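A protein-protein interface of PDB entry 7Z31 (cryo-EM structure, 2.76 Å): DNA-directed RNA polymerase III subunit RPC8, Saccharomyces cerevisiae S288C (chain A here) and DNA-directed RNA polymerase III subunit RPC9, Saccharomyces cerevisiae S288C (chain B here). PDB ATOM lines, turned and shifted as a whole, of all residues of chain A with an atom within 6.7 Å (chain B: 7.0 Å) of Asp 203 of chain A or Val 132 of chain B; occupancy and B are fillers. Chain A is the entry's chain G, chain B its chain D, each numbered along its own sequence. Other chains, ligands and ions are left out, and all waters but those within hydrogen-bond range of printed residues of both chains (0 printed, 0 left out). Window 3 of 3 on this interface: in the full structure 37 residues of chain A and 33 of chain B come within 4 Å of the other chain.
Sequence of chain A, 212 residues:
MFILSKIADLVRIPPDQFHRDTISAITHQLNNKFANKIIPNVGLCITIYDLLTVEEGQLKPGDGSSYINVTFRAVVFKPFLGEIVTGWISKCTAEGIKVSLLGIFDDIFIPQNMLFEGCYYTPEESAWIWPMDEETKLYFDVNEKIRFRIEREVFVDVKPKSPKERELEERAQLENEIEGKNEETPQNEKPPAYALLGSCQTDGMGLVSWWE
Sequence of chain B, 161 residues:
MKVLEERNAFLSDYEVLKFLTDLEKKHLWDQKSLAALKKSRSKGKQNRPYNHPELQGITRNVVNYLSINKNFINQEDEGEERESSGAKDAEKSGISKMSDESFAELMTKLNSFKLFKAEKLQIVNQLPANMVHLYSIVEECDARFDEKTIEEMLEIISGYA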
ATOM      1  N   PHE A 116      14.505  14.932  -4.954  1.00  0.00           N
ATOM      2  CA  PHE A 116      14.594  13.486  -5.116  1.00  0.00           C
ATOM      3  C   PHE A 116      13.484  12.994  -6.036  1.00  0.00           C
ATOM      4  O   PHE A 116      12.324  13.395  -5.896  1.00  0.00           O
ATOM      5  CB  PHE A 116      14.501  12.792  -3.756  1.00  0.00           C
ATOM      6  CG  PHE A 116      15.835  12.537  -3.105  1.00  0.00           C
ATOM      7  CD1 PHE A 116      16.754  11.681  -3.688  1.00  0.00           C
ATOM      8  CD2 PHE A 116      16.156  13.129  -1.894  1.00  0.00           C
ATOM      9  CE1 PHE A 116      17.976  11.435  -3.088  1.00  0.00           C
ATOM     10  CE2 PHE A 116      17.381  12.885  -1.288  1.00  0.00           C
ATOM     11  CZ  PHE A 116      18.291  12.037  -1.889  1.00  0.00           C
ATOM     12  N   ARG A 147      18.694  18.146   5.055  1.00  0.00           N
ATOM     13  CA  ARG A 147      20.011  18.447   4.510  1.00  0.00           C
ATOM     14  C   ARG A 147      19.900  18.609   3.001  1.00  0.00           C
ATOM     15  O   ARG A 147      19.292  17.773   2.324  1.00  0.00           O
ATOM     16  CB  ARG A 147      21.022  17.351   4.863  1.00  0.00           C
ATOM     17  CG  ARG A 147      22.334  17.440   4.090  1.00  0.00           C
ATOM     18  CD  ARG A 147      23.501  16.811   4.850  1.00  0.00           C
ATOM     19  NE  ARG A 147      23.303  15.398   5.147  1.00  0.00           N
ATOM     20  CZ  ARG A 147      22.954  14.922   6.334  1.00  0.00           C
ATOM     21  NH1 ARG A 147      22.755  15.721   7.369  1.00  0.00           N
ATOM     22  NH2 ARG A 147      22.804  13.611   6.487  1.00  0.00           N
ATOM     23  N   CYS A 200      18.825  17.821  -3.546  1.00  0.00           N
ATOM     24  CA  CYS A 200      18.817  16.589  -2.769  1.00  0.00           C
ATOM     25  C   CYS A 200      19.192  15.416  -3.660  1.00  0.00           C
ATOM     26  O   CYS A 200      18.496  14.398  -3.706  1.00  0.00           O
ATOM     27  CB  CYS A 200      17.459  16.362  -2.109  1.00  0.00           C
ATOM     28  SG  CYS A 200      17.059  17.556  -0.819  1.00  0.00           S
ATOM     29  N   GLN A 201      20.291  15.558  -4.405  1.00  0.00           N
ATOM     30  CA  GLN A 201      20.707  14.524  -5.343  1.00  0.00           C
ATOM     31  C   GLN A 201      21.687  13.525  -4.742  1.00  0.00           C
ATOM     32  O   GLN A 201      21.813  12.413  -5.265  1.00  0.00           O
ATOM     33  CB  GLN A 201      21.330  15.171  -6.582  1.00  0.00           C
ATOM     34  CG  GLN A 201      20.401  15.216  -7.782  1.00  0.00           C
ATOM     35  CD  GLN A 201      20.254  13.860  -8.435  1.00  0.00           C
ATOM     36  OE1 GLN A 201      19.258  13.577  -9.102  1.00  0.00           O
ATOM     37  NE2 GLN A 201      21.256  13.008  -8.247  1.00  0.00           N
ATOM     38  N   THR A 202      22.366  13.879  -3.655  1.00  0.00           N
ATOM     39  CA  THR A 202      23.414  13.042  -3.088  1.00  0.00           C
ATOM     40  C   THR A 202      22.892  12.266  -1.887  1.00  0.00           C
ATOM     41  O   THR A 202      22.160  12.807  -1.054  1.00  0.00           O
ATOM     42  CB  THR A 202      24.621  13.887  -2.679  1.00  0.00           C
ATOM     43  OG1 THR A 202      25.086  14.625  -3.814  1.00  0.00           O
ATOM     44  CG2 THR A 202      25.753  12.999  -2.168  1.00  0.00           C
ATOM     45  N   ASP A 203      23.274  10.992  -1.810  1.00  0.00           N
ATOM     46  CA  ASP A 203      22.877  10.149  -0.691  1.00  0.00           C
ATOM     47  C   ASP A 203      23.359  10.742   0.628  1.00  0.00           C
ATOM     48  O   ASP A 203      24.460  11.292   0.718  1.00  0.00           O
ATOM     49  CB  ASP A 203      23.435   8.736  -0.872  1.00  0.00           C
ATOM     50  CG  ASP A 203      24.953   8.707  -0.938  1.00  0.00           C
ATOM     51  OD1 ASP A 203      25.561   9.744  -1.274  1.00  0.00           O
ATOM     52  OD2 ASP A 203      25.541   7.641  -0.661  1.00  0.00           O
ATOM     53  N   GLY A 204      22.514  10.640   1.653  1.00  0.00           N
ATOM     54  CA  GLY A 204      22.786  11.192   2.957  1.00  0.00           C
ATOM     55  C   GLY A 204      22.113  12.524   3.218  1.00  0.00           C
ATOM     56  O   GLY A 204      21.964  12.913   4.382  1.00  0.00           O
ATOM     57  N   MET A 205      21.714  13.238   2.171  1.00  0.00           N
ATOM     58  CA  MET A 205      20.982  14.481   2.363  1.00  0.00           C
ATOM     59  C   MET A 205      19.503  14.197   2.601  1.00  0.00           C
ATOM     60  O   MET A 205      18.897  13.358   1.928  1.00  0.00           O
ATOM     61  CB  MET A 205      21.164  15.400   1.155  1.00  0.00           C
ATOM     62  CG  MET A 205      22.619  15.769   0.903  1.00  0.00           C
ATOM     63  SD  MET A 205      22.871  17.246  -0.098  1.00  0.00           S
ATOM     64  CE  MET A 205      22.386  16.656  -1.717  1.00  0.00           C
ATOM     65  N   TRP A 210      19.686   8.909   8.959  1.00  0.00           N
ATOM     66  CA  TRP A 210      19.034   7.879   8.160  1.00  0.00           C
ATOM     67  C   TRP A 210      19.356   6.473   8.647  1.00  0.00           C
ATOM     68  O   TRP A 210      18.481   5.600   8.622  1.00  0.00           O
ATOM     69  CB  TRP A 210      19.423   8.000   6.680  1.00  0.00           C
ATOM     70  CG  TRP A 210      18.726   9.097   5.900  1.00  0.00           C
ATOM     71  CD1 TRP A 210      19.306   9.946   5.001  1.00  0.00           C
ATOM     72  CD2 TRP A 210      17.332   9.451   5.940  1.00  0.00           C
ATOM     73  NE1 TRP A 210      18.367  10.803   4.482  1.00  0.00           N
ATOM     74  CE2 TRP A 210      17.149  10.521   5.042  1.00  0.00           C
ATOM     75  CE3 TRP A 210      16.225   8.968   6.646  1.00  0.00           C
ATOM     76  CZ2 TRP A 210      15.903  11.118   4.833  1.00  0.00           C
ATOM     77  CZ3 TRP A 210      14.991   9.562   6.438  1.00  0.00           C
ATOM     78  CH2 TRP A 210      14.841  10.626   5.541  1.00  0.00           C
ATOM     79  N   TRP A 211      20.590   6.234   9.095  1.00  0.00           N
ATOM     80  CA  TRP A 211      21.011   4.922   9.567  1.00  0.00           C
ATOM     81  C   TRP A 211      21.829   5.080  10.843  1.00  0.00           C
ATOM     82  O   TRP A 211      22.225   6.185  11.225  1.00  0.00           O
ATOM     83  CB  TRP A 211      21.829   4.170   8.511  1.00  0.00           C
ATOM     84  CG  TRP A 211      21.312   4.312   7.109  1.00  0.00           C
ATOM     85  CD1 TRP A 211      20.267   3.639   6.544  1.00  0.00           C
ATOM     86  CD2 TRP A 211      21.836   5.170   6.089  1.00  0.00           C
ATOM     87  NE1 TRP A 211      20.102   4.034   5.236  1.00  0.00           N
ATOM     88  CE2 TRP A 211      21.055   4.972   4.933  1.00  0.00           C
ATOM     89  CE3 TRP A 211      22.888   6.092   6.042  1.00  0.00           C
ATOM     90  CZ2 TRP A 211      21.294   5.658   3.743  1.00  0.00           C
ATOM     91  CZ3 TRP A 211      23.122   6.772   4.860  1.00  0.00           C
ATOM     92  CH2 TRP A 211      22.328   6.554   3.728  1.00  0.00           C
ATOM     93  N   LEU B 127      28.274  18.149  10.200  1.00  0.00           N
ATOM     94  CA  LEU B 127      28.353  16.876   9.494  1.00  0.00           C
ATOM     95  C   LEU B 127      29.460  15.949   9.990  1.00  0.00           C
ATOM     96  O   LEU B 127      30.249  15.454   9.175  1.00  0.00           O
ATOM     97  CB  LEU B 127      28.535  17.140   8.000  1.00  0.00           C
ATOM     98  CG  LEU B 127      27.442  17.965   7.326  1.00  0.00           C
ATOM     99  CD1 LEU B 127      27.861  18.340   5.924  1.00  0.00           C
ATOM    100  CD2 LEU B 127      26.132  17.195   7.303  1.00  0.00           C
ATOM    101  N   ALA B 129      30.623  12.233  12.151  1.00  0.00           N
ATOM    102  CA  ALA B 129      30.139  10.875  12.410  1.00  0.00           C
ATOM    103  C   ALA B 129      29.476  10.239  11.189  1.00  0.00           C
ATOM    104  O   ALA B 129      28.505   9.489  11.325  1.00  0.00           O
ATOM    105  CB  ALA B 129      29.180  10.848  13.605  1.00  0.00           C
ATOM    106  N   ASN B 130      29.986  10.523   9.992  1.00  0.00           N
ATOM    107  CA  ASN B 130      29.520   9.840   8.793  1.00  0.00           C
ATOM    108  C   ASN B 130      30.469  10.132   7.640  1.00  0.00           C
ATOM    109  O   ASN B 130      30.907  11.272   7.467  1.00  0.00           O
ATOM    110  CB  ASN B 130      28.099  10.263   8.409  1.00  0.00           C
ATOM    111  CG  ASN B 130      27.526   9.406   7.308  1.00  0.00           C
ATOM    112  OD1 ASN B 130      27.849   8.224   7.201  1.00  0.00           O
ATOM    113  ND2 ASN B 130      26.679   9.995   6.474  1.00  0.00           N
ATOM    114  N   MET B 131      30.770   9.097   6.849  1.00  0.00           N
ATOM    115  CA  MET B 131      31.592   9.294   5.659  1.00  0.00           C
ATOM    116  C   MET B 131      30.834  10.059   4.584  1.00  0.00           C
ATOM    117  O   MET B 131      31.404  10.932   3.917  1.00  0.00           O
ATOM    118  CB  MET B 131      32.070   7.946   5.116  1.00  0.00           C
ATOM    119  CG  MET B 131      33.106   8.041   3.998  1.00  0.00           C
ATOM    120  SD  MET B 131      32.421   8.325   2.351  1.00  0.00           S
ATOM    121  CE  MET B 131      33.911   8.334   1.356  1.00  0.00           C
ATOM    122  N   VAL B 132      29.547   9.747   4.402  1.00  0.00           N
ATOM    123  CA  VAL B 132      28.782  10.325   3.300  1.00  0.00           C
ATOM    124  C   VAL B 132      28.622  11.832   3.470  1.00  0.00           C
ATOM    125  O   VAL B 132      28.518  12.570   2.480  1.00  0.00           O
ATOM    126  CB  VAL B 132      27.424   9.604   3.172  1.00  0.00           C
ATOM    127  CG1 VAL B 132      26.264  10.582   3.288  1.00  0.00           C
ATOM    128  CG2 VAL B 132      27.358   8.835   1.858  1.00  0.00           C
ATOM    129  N   HIS B 133      28.613  12.315   4.715  1.00  0.00           N
ATOM    130  CA  HIS B 133      28.570  13.755   4.946  1.00  0.00           C
ATOM    131  C   HIS B 133      29.736  14.448   4.257  1.00  0.00           C
ATOM    132  O   HIS B 133      29.545  15.389   3.480  1.00  0.00           O
ATOM    133  CB  HIS B 133      28.592  14.050   6.443  1.00  0.00           C
ATOM    134  CG  HIS B 133      27.349  13.635   7.164  1.00  0.00           C
ATOM    135  ND1 HIS B 133      27.197  13.781   8.525  1.00  0.00           N
ATOM    136  CD2 HIS B 133      26.198  13.083   6.713  1.00  0.00           C
ATOM    137  CE1 HIS B 133      26.009  13.331   8.884  1.00  0.00           C
ATOM    138  NE2 HIS B 133      25.383  12.900   7.804  1.00  0.00           N
ATOM    139  N   LEU B 134      30.958  13.974   4.511  1.00  0.00           N
ATOM    140  CA  LEU B 134      32.115  14.510   3.805  1.00  0.00           C
ATOM    141  C   LEU B 134      32.062  14.178   2.319  1.00  0.00           C
ATOM    142  O   LEU B 134      32.584  14.938   1.497  1.00  0.00           O
ATOM    143  CB  LEU B 134      33.402  13.983   4.445  1.00  0.00           C
ATOM    144  CG  LEU B 134      34.711  14.041   3.655  1.00  0.00           C
ATOM    145  CD1 LEU B 134      35.868  14.465   4.540  1.00  0.00           C
ATOM    146  CD2 LEU B 134      34.999  12.691   3.030  1.00  0.00           C
ATOM    147  N   TYR B 135      31.426  13.062   1.953  1.00  0.00           N
ATOM    148  CA  TYR B 135      31.271  12.730   0.542  1.00  0.00           C
ATOM    149  C   TYR B 135      30.400  13.744  -0.186  1.00  0.00           C
ATOM    150  O   TYR B 135      30.446  13.818  -1.419  1.00  0.00           O
ATOM    151  CB  TYR B 135      30.688  11.326   0.395  1.00  0.00           C
ATOM    152  CG  TYR B 135      30.785  10.771  -1.007  1.00  0.00           C
ATOM    153  CD1 TYR B 135      32.018  10.629  -1.631  1.00  0.00           C
ATOM    154  CD2 TYR B 135      29.648  10.380  -1.703  1.00  0.00           C
ATOM    155  CE1 TYR B 135      32.115  10.121  -2.912  1.00  0.00           C
ATOM    156  CE2 TYR B 135      29.737   9.866  -2.984  1.00  0.00           C
ATOM    157  CZ  TYR B 135      30.974   9.739  -3.584  1.00  0.00           C
ATOM    158  OH  TYR B 135      31.071   9.230  -4.860  1.00  0.00           O
ATOM    159  N   SER B 136      29.592  14.505   0.547  1.00  0.00           N
ATOM    160  CA  SER B 136      28.905  15.665  -0.009  1.00  0.00           C
ATOM    161  C   SER B 136      29.671  16.961   0.215  1.00  0.00           C
ATOM    162  O   SER B 136      29.553  17.890  -0.589  1.00  0.00           O
ATOM    163  CB  SER B 136      27.503  15.793   0.596  1.00  0.00           C
ATOM    164  OG  SER B 136      26.765  16.839  -0.016  1.00  0.00           O
ATOM    165  N   ILE B 137      30.453  17.031   1.294  1.00  0.00           N
ATOM    166  CA  ILE B 137      31.245  18.225   1.581  1.00  0.00           C
ATOM    167  C   ILE B 137      32.269  18.463   0.478  1.00  0.00           C
ATOM    168  O   ILE B 137      32.374  19.568  -0.069  1.00  0.00           O
ATOM    169  CB  ILE B 137      31.917  18.102   2.959  1.00  0.00           C
ATOM    170  CG1 ILE B 137      30.858  18.162   4.054  1.00  0.00           C
ATOM    171  CG2 ILE B 137      32.946  19.203   3.149  1.00  0.00           C
ATOM    172  CD1 ILE B 137      31.311  17.621   5.388  1.00  0.00           C
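A ring nitrogen (NE2) of His 133 of chain B is in hydrogen-bond range of the guanidinium group of Arg 147 of chain A.
Hydrophobic or aromatic side chains of chain B within 4 Å of the printed part of chain A: Leu 127, Val 132 and His 133. Along chain B the printed residues that touch a printed residue of chain A span positions 127 to 136. Hydrophobic or aromatic side chains of chain A within 4 Å of the printed part of chain B: Met 205. Among the printed residues, 5 pairs touch across the chains. Among the printed residues, no Asp or Glu carboxylate lies within 4 Å of a Lys or Arg side-chain nitrogen of the other chain.
Among the printed residues, pairs that only touch across the chains: Asp 203 of chain A with Val 132 of chain B, Gly 204 of chain A with Val 132 of chain B, Arg 147 of chain A with Leu 127 of chain B and Met 205 of chain A with Ser 136 of chain B.
The backbone carbonyl oxygen (O) of Gly 204 of chain A lies within hydrogen-bond range of the guanidinium group (NE) of Arg 147 of chain A, 2.9 Å away. A ring nitrogen (NE2) of His 133 of chain B lies close to the side-chain amide nitrogen (ND2) of Asn 130 of chain B (3.4 Å).
Of the printed residues of chain B, Arg 147 of chain A touches Leu 127 (3.6 Å) and His 133 (3.0 Å). Gln 201 of chain A touches none of the printed residues of chain B. Asp 203 of chain A touches one residue of chain B. Ala 129 of chain B touches none of the printed residues of chain A. Val 132 of chain B touches just these residues of chain A: Asp 203 (3.2 Å) and Gly 204 (3.5 Å). Printed residues of chain A within 4 Å of His 133 of chain B: Arg 147 (3.0 Å). The nearest residue of chain B that does not touch Asp 203 of chain A is Tyr 135 of chain B (4.2 Å). The nearest residue of chain A that does not touch Val 132 of chain B is Trp 211 of chain A (5.2 Å).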
